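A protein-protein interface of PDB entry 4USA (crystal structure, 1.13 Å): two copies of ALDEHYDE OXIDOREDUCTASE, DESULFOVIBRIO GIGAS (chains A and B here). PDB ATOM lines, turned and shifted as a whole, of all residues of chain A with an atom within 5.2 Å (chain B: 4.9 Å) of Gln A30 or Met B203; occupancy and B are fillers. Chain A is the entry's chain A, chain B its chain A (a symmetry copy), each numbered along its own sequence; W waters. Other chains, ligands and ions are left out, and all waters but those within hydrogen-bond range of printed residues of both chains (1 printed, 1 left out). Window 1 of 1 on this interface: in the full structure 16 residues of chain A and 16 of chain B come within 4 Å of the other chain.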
ATOM      1  N   MET A   1      17.042 -21.336   3.053  1.00  0.00           N
ATOM      2  CA  MET A   1      16.804 -21.239   1.561  1.00  0.00           C
ATOM      3  C   MET A   1      17.418 -22.456   0.958  1.00  0.00           C
ATOM      4  O   MET A   1      18.356 -23.038   1.524  1.00  0.00           O
ATOM      5  CB  MET A   1      17.461 -19.938   1.011  1.00  0.00           C
ATOM      6  CG  MET A   1      17.686 -19.925  -0.505  1.00  0.00           C
ATOM      7  SD  MET A   1      18.136 -18.289  -1.089  1.00  0.00           S
ATOM      8  CE  MET A   1      16.581 -17.442  -1.214  1.00  0.00           C
ATOM      9  N   PHE A  16      16.020 -20.401  -6.506  1.00  0.00           N
ATOM     10  CA  PHE A  16      16.387 -20.173  -5.116  1.00  0.00           C
ATOM     11  C   PHE A  16      15.125 -19.831  -4.350  1.00  0.00           C
ATOM     12  O   PHE A  16      14.506 -18.804  -4.640  1.00  0.00           O
ATOM     13  CB  PHE A  16      17.445 -19.074  -5.050  1.00  0.00           C
ATOM     14  CG  PHE A  16      18.723 -19.550  -5.687  1.00  0.00           C
ATOM     15  CD1 PHE A  16      19.638 -20.249  -4.928  1.00  0.00           C
ATOM     16  CD2 PHE A  16      18.949 -19.401  -7.041  1.00  0.00           C
ATOM     17  CE1 PHE A  16      20.770 -20.789  -5.516  1.00  0.00           C
ATOM     18  CE2 PHE A  16      20.067 -19.949  -7.624  1.00  0.00           C
ATOM     19  CZ  PHE A  16      20.975 -20.635  -6.853  1.00  0.00           C
ATOM     20  N   VAL A  17      14.725 -20.724  -3.456  1.00  0.00           N
ATOM     21  CA  VAL A  17      13.434 -20.638  -2.806  1.00  0.00           C
ATOM     22  C   VAL A  17      13.513 -20.938  -1.335  1.00  0.00           C
ATOM     23  O   VAL A  17      14.415 -21.616  -0.862  1.00  0.00           O
ATOM     24  CB  VAL A  17      12.395 -21.573  -3.469  1.00  0.00           C
ATOM     25  CG1 VAL A  17      12.086 -21.101  -4.884  1.00  0.00           C
ATOM     26  CG2 VAL A  17      12.842 -23.032  -3.456  1.00  0.00           C
ATOM     27  N   ASP A  25       3.261 -18.510  -5.548  1.00  0.00           N
ATOM     28  CA  ASP A  25       4.050 -17.293  -5.357  1.00  0.00           C
ATOM     29  C   ASP A  25       5.368 -17.359  -6.087  1.00  0.00           C
ATOM     30  O   ASP A  25       5.804 -16.386  -6.700  1.00  0.00           O
ATOM     31  CB  ASP A  25       4.293 -17.044  -3.874  1.00  0.00           C
ATOM     32  CG  ASP A  25       3.033 -16.651  -3.129  1.00  0.00           C
ATOM     33  OD1 ASP A  25       2.141 -16.036  -3.723  1.00  0.00           O
ATOM     34  OD2 ASP A  25       2.944 -16.932  -1.930  1.00  0.00           O
ATOM     35  N   VAL A  26       6.035 -18.505  -6.018  1.00  0.00           N
ATOM     36  CA  VAL A  26       7.305 -18.647  -6.726  1.00  0.00           C
ATOM     37  C   VAL A  26       7.100 -18.416  -8.216  1.00  0.00           C
ATOM     38  O   VAL A  26       7.837 -17.666  -8.847  1.00  0.00           O
ATOM     39  CB  VAL A  26       7.940 -20.002  -6.422  1.00  0.00           C
ATOM     40  CG1 VAL A  26       9.175 -20.214  -7.263  1.00  0.00           C
ATOM     41  CG2 VAL A  26       8.294 -20.098  -4.930  1.00  0.00           C
ATOM     42  N   LEU A  27       6.122 -19.104  -8.792  1.00  0.00           N
ATOM     43  CA  LEU A  27       5.884 -19.001 -10.215  1.00  0.00           C
ATOM     44  C   LEU A  27       5.497 -17.582 -10.619  1.00  0.00           C
ATOM     45  O   LEU A  27       6.034 -17.035 -11.584  1.00  0.00           O
ATOM     46  CB  LEU A  27       4.826 -20.007 -10.652  1.00  0.00           C
ATOM     47  CG  LEU A  27       5.241 -21.491 -10.509  1.00  0.00           C
ATOM     48  CD1 LEU A  27       4.056 -22.387 -10.852  1.00  0.00           C
ATOM     49  CD2 LEU A  27       6.427 -21.862 -11.342  1.00  0.00           C
ATOM     50  N   ARG A  28       4.530 -17.000  -9.898  1.00  0.00           N
ATOM     51  CA  ARG A  28       4.052 -15.656 -10.273  1.00  0.00           C
ATOM     52  C   ARG A  28       5.057 -14.563 -10.014  1.00  0.00           C
ATOM     53  O   ARG A  28       5.294 -13.701 -10.864  1.00  0.00           O
ATOM     54  CB  ARG A  28       2.751 -15.329  -9.533  1.00  0.00           C
ATOM     55  CG  ARG A  28       1.552 -16.134  -9.974  1.00  0.00           C
ATOM     56  CD  ARG A  28       0.315 -15.862  -9.124  1.00  0.00           C
ATOM     57  NE  ARG A  28      -0.092 -14.452  -9.113  1.00  0.00           N
ATOM     58  CZ  ARG A  28      -0.693 -13.817 -10.115  1.00  0.00           C
ATOM     59  NH1 ARG A  28      -0.988 -14.445 -11.241  1.00  0.00           N
ATOM     60  NH2 ARG A  28      -0.965 -12.522  -9.990  1.00  0.00           N
ATOM     61  N   GLN A  29       5.615 -14.579  -8.802  1.00  0.00           N
ATOM     62  CA  GLN A  29       6.451 -13.473  -8.325  1.00  0.00           C
ATOM     63  C   GLN A  29       7.904 -13.630  -8.706  1.00  0.00           C
ATOM     64  O   GLN A  29       8.532 -12.708  -9.217  1.00  0.00           O
ATOM     65  CB  GLN A  29       6.293 -13.306  -6.834  1.00  0.00           C
ATOM     66  CG  GLN A  29       4.861 -13.069  -6.412  1.00  0.00           C
ATOM     67  CD  GLN A  29       4.678 -12.721  -4.985  1.00  0.00           C
ATOM     68  OE1 GLN A  29       5.428 -11.907  -4.444  1.00  0.00           O
ATOM     69  NE2 GLN A  29       3.595 -13.212  -4.405  1.00  0.00           N
ATOM     70  N   GLN A  30       8.495 -14.775  -8.409  1.00  0.00           N
ATOM     71  CA  GLN A  30       9.901 -14.955  -8.722  1.00  0.00           C
ATOM     72  C   GLN A  30      10.120 -15.142 -10.212  1.00  0.00           C
ATOM     73  O   GLN A  30      11.111 -14.605 -10.749  1.00  0.00           O
ATOM     74  CB  GLN A  30      10.510 -16.093  -7.909  1.00  0.00           C
ATOM     75  CG  GLN A  30      10.514 -15.783  -6.429  1.00  0.00           C
ATOM     76  CD  GLN A  30      11.074 -16.879  -5.559  1.00  0.00           C
ATOM     77  OE1 GLN A  30      10.413 -17.370  -4.636  1.00  0.00           O
ATOM     78  NE2 GLN A  30      12.309 -17.277  -5.812  1.00  0.00           N
ATOM     79  N   LEU A  31       9.233 -15.883 -10.890  1.00  0.00           N
ATOM     80  CA  LEU A  31       9.446 -16.207 -12.300  1.00  0.00           C
ATOM     81  C   LEU A  31       8.578 -15.415 -13.252  1.00  0.00           C
ATOM     82  O   LEU A  31       8.736 -15.560 -14.456  1.00  0.00           O
ATOM     83  CB  LEU A  31       9.280 -17.702 -12.560  1.00  0.00           C
ATOM     84  CG  LEU A  31      10.218 -18.618 -11.746  1.00  0.00           C
ATOM     85  CD1 LEU A  31      10.003 -20.081 -12.135  1.00  0.00           C
ATOM     86  CD2 LEU A  31      11.665 -18.181 -11.852  1.00  0.00           C
ATOM     87  N   GLY A  32       7.668 -14.594 -12.743  1.00  0.00           N
ATOM     88  CA  GLY A  32       6.857 -13.752 -13.625  1.00  0.00           C
ATOM     89  C   GLY A  32       5.763 -14.467 -14.395  1.00  0.00           C
ATOM     90  O   GLY A  32       5.232 -13.896 -15.360  1.00  0.00           O
ATOM     91  N   LEU B 199      19.645 -13.966 -11.357  1.00  0.00           N
ATOM     92  CA  LEU B 199      19.237 -14.761 -10.209  1.00  0.00           C
ATOM     93  C   LEU B 199      18.766 -13.862  -9.070  1.00  0.00           C
ATOM     94  O   LEU B 199      17.779 -14.155  -8.402  1.00  0.00           O
ATOM     95  CB  LEU B 199      20.387 -15.666  -9.784  1.00  0.00           C
ATOM     96  CG  LEU B 199      20.746 -16.768 -10.805  1.00  0.00           C
ATOM     97  CD1 LEU B 199      22.040 -17.447 -10.430  1.00  0.00           C
ATOM     98  CD2 LEU B 199      19.621 -17.779 -10.972  1.00  0.00           C
ATOM     99  N   GLY B 200      19.442 -12.726  -8.860  1.00  0.00           N
ATOM    100  CA  GLY B 200      19.006 -11.803  -7.848  1.00  0.00           C
ATOM    101  C   GLY B 200      17.590 -11.309  -8.033  1.00  0.00           C
ATOM    102  O   GLY B 200      16.835 -11.225  -7.082  1.00  0.00           O
ATOM    103  N   LEU B 201      17.186 -11.072  -9.273  1.00  0.00           N
ATOM    104  CA  LEU B 201      15.815 -10.625  -9.539  1.00  0.00           C
ATOM    105  C   LEU B 201      14.805 -11.732  -9.307  1.00  0.00           C
ATOM    106  O   LEU B 201      13.616 -11.435  -9.144  1.00  0.00           O
ATOM    107  CB  LEU B 201      15.706 -10.097 -10.955  1.00  0.00           C
ATOM    108  CG  LEU B 201      16.448  -8.806 -11.244  1.00  0.00           C
ATOM    109  CD1 LEU B 201      16.179  -8.354 -12.668  1.00  0.00           C
ATOM    110  CD2 LEU B 201      16.096  -7.698 -10.283  1.00  0.00           C
ATOM    111  N   LYS B 202      15.247 -12.971  -9.321  1.00  0.00           N
ATOM    112  CA  LYS B 202      14.387 -14.144  -9.215  1.00  0.00           C
ATOM    113  C   LYS B 202      14.460 -14.778  -7.836  1.00  0.00           C
ATOM    114  O   LYS B 202      13.940 -15.870  -7.622  1.00  0.00           O
ATOM    115  CB  LYS B 202      14.740 -15.146 -10.290  1.00  0.00           C
ATOM    116  CG  LYS B 202      14.554 -14.533 -11.672  1.00  0.00           C
ATOM    117  CD  LYS B 202      14.841 -15.474 -12.821  1.00  0.00           C
ATOM    118  CE  LYS B 202      14.736 -14.691 -14.107  1.00  0.00           C
ATOM    119  NZ  LYS B 202      15.014 -15.522 -15.283  1.00  0.00           N
ATOM    120  N   MET B 203      15.111 -14.110  -6.883  1.00  0.00           N
ATOM    121  CA  MET B 203      15.199 -14.573  -5.514  1.00  0.00           C
ATOM    122  C   MET B 203      13.932 -14.087  -4.791  1.00  0.00           C
ATOM    123  O   MET B 203      13.264 -13.129  -5.182  1.00  0.00           O
ATOM    124  CB  MET B 203      16.497 -14.077  -4.845  1.00  0.00           C
ATOM    125  CG  MET B 203      17.715 -14.894  -5.259  1.00  0.00           C
ATOM    126  SD  MET B 203      19.279 -14.210  -4.667  1.00  0.00           S
ATOM    127  CE  MET B 203      19.292 -14.856  -3.025  1.00  0.00           C
ATOM    128  N   PRO B 204      13.646 -14.693  -3.686  1.00  0.00           N
ATOM    129  CA  PRO B 204      12.383 -14.358  -3.018  1.00  0.00           C
ATOM    130  C   PRO B 204      12.391 -13.064  -2.281  1.00  0.00           C
ATOM    131  O   PRO B 204      13.444 -12.580  -1.947  1.00  0.00           O
ATOM    132  CB  PRO B 204      12.197 -15.470  -2.052  1.00  0.00           C
ATOM    133  CG  PRO B 204      13.449 -16.111  -1.802  1.00  0.00           C
ATOM    134  CD  PRO B 204      14.343 -15.774  -3.026  1.00  0.00           C
ATOM    135  N   ALA B 205      11.194 -12.559  -1.954  1.00  0.00           N
ATOM    136  CA  ALA B 205      11.019 -11.278  -1.267  1.00  0.00           C
ATOM    137  C   ALA B 205      11.840 -11.108   0.018  1.00  0.00           C
ATOM    138  O   ALA B 205      12.225  -9.983   0.318  1.00  0.00           O
ATOM    139  CB  ALA B 205       9.554 -11.031  -0.979  1.00  0.00           C
ATOM    140  N   THR B 207      14.851 -11.695   0.521  1.00  0.00           N
ATOM    141  CA  THR B 207      16.251 -11.480   0.167  1.00  0.00           C
ATOM    142  C   THR B 207      16.631 -10.031   0.470  1.00  0.00           C
ATOM    143  O   THR B 207      15.926  -9.093   0.105  1.00  0.00           O
ATOM    144  CB  THR B 207      16.504 -11.824  -1.295  1.00  0.00           C
ATOM    145  OG1 THR B 207      16.154 -13.186  -1.528  1.00  0.00           O
ATOM    146  CG2 THR B 207      17.938 -11.603  -1.690  1.00  0.00           C
ATOM    147  N   PHE B 374      25.814 -13.915  -4.364  1.00  0.00           N
ATOM    148  CA  PHE B 374      24.808 -13.998  -3.327  1.00  0.00           C
ATOM    149  C   PHE B 374      25.119 -15.129  -2.389  1.00  0.00           C
ATOM    150  O   PHE B 374      25.930 -15.999  -2.688  1.00  0.00           O
ATOM    151  CB  PHE B 374      23.382 -14.043  -3.930  1.00  0.00           C
ATOM    152  CG  PHE B 374      23.096 -15.207  -4.822  1.00  0.00           C
ATOM    153  CD1 PHE B 374      22.554 -16.393  -4.328  1.00  0.00           C
ATOM    154  CD2 PHE B 374      23.302 -15.129  -6.187  1.00  0.00           C
ATOM    155  CE1 PHE B 374      22.230 -17.431  -5.165  1.00  0.00           C
ATOM    156  CE2 PHE B 374      22.954 -16.170  -7.034  1.00  0.00           C
ATOM    157  CZ  PHE B 374      22.418 -17.306  -6.524  1.00  0.00           C
ATOM    158  N   PRO B 443      18.847 -14.564   3.081  1.00  0.00           N
ATOM    159  CA  PRO B 443      19.552 -14.513   1.791  1.00  0.00           C
ATOM    160  C   PRO B 443      19.985 -13.083   1.516  1.00  0.00           C
ATOM    161  O   PRO B 443      19.242 -12.143   1.831  1.00  0.00           O
ATOM    162  CB  PRO B 443      18.490 -14.980   0.775  1.00  0.00           C
ATOM    163  CG  PRO B 443      17.462 -15.713   1.609  1.00  0.00           C
ATOM    164  CD  PRO B 443      17.446 -14.958   2.894  1.00  0.00           C
ATOM    165  N   VAL B 444      21.171 -12.936   0.919  1.00  0.00           N
ATOM    166  CA  VAL B 444      21.715 -11.639   0.589  1.00  0.00           C
ATOM    167  C   VAL B 444      22.265 -11.681  -0.826  1.00  0.00           C
ATOM    168  O   VAL B 444      22.778 -12.690  -1.282  1.00  0.00           O
ATOM    169  CB  VAL B 444      22.818 -11.181   1.571  1.00  0.00           C
ATOM    170  CG1 VAL B 444      22.280 -11.154   2.993  1.00  0.00           C
ATOM    171  CG2 VAL B 444      24.041 -12.093   1.500  1.00  0.00           C
ATOM    172  N   HIS B 445      22.188 -10.535  -1.504  1.00  0.00           N
ATOM    173  CA  HIS B 445      22.643 -10.426  -2.896  1.00  0.00           C
ATOM    174  C   HIS B 445      23.393  -9.121  -3.059  1.00  0.00           C
ATOM    175  O   HIS B 445      22.909  -8.069  -2.618  1.00  0.00           O
ATOM    176  CB  HIS B 445      21.428 -10.503  -3.830  1.00  0.00           C
ATOM    177  CG  HIS B 445      21.794 -10.573  -5.271  1.00  0.00           C
ATOM    178  ND1 HIS B 445      22.101  -9.447  -5.998  1.00  0.00           N
ATOM    179  CD2 HIS B 445      21.877 -11.623  -6.112  1.00  0.00           C
ATOM    180  CE1 HIS B 445      22.376  -9.829  -7.238  1.00  0.00           C
ATOM    181  NE2 HIS B 445      22.250 -11.142  -7.344  1.00  0.00           N
HETATM  182  O   HOH W   1      15.345 -18.303  -8.342  1.00  0.00           O
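NE2 of Gln A30 lies within hydrogen-bond range of O of Lys B202.
Met A1 touches Pro B204. Pro B443 touches Met A1 (CG to CE, 3.4 Å). Phe A16 touches Pro B204 (O to CD, 3.4 Å). Phe A16 touches Phe B374 (CZ to CZ, 3.6 Å). Met B203 touches Gln A30 (C to NE2, 3.7 Å). Gln A30 touches Pro B204.
Of the printed residues of chain B, Met A1 touches Pro B204 (3.3 Å) and Pro B443 (3.4 Å). Printed residues of chain B within 4 Å of Phe A16: Pro B204 and Phe B374. Of the printed residues of chain B, Gln A30 touches Lys B202 (2.8 Å), Met B203 (3.7 Å) and Pro B204 (3.6 Å). Gly B200 touches none of the printed residues of chain A. Of the printed residues of chain A, Met B203 touches Gln A30 (3.7 Å). Of the printed residues of chain A, Phe B374 touches Phe A16. Of the printed residues of chain A, Pro B443 touches Met A1 (3.4 Å). The nearest printed residue of chain B that does not touch Gln A30 is Leu B201 (4.3 Å). The nearest residue of chain A that does not touch Met B203 is Met A1 (4.1 Å).
Of the 11 printed residues of chain A, 3 touch a printed residue of chain B. Printed residues of chain A that touch a printed residue of chain B: Met A1, Phe A16 and Gln A30. Along chain A the printed residues that touch a printed residue of chain B span positions 1 to 30. Among the printed residues, 7 pairs touch across the chains.
O of Pro B204 sits at hydrogen-bond distance from OG1 of Thr B207 (2.8 Å). The side-chain amide nitrogen (NE2) of Gln A30 is in hydrogen-bond range of the backbone carbonyl oxygen (O) of Phe A16, at 2.9 Å.
Water W1 lies within hydrogen-bond range of the backbone NH of Phe A16 and the backbone carbonyl oxygen of Lys B202.
No position is printed for both chains. Of the 7 pairs that touch across the chains among the printed residues, none has its exchanged pair printed and touching as well.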
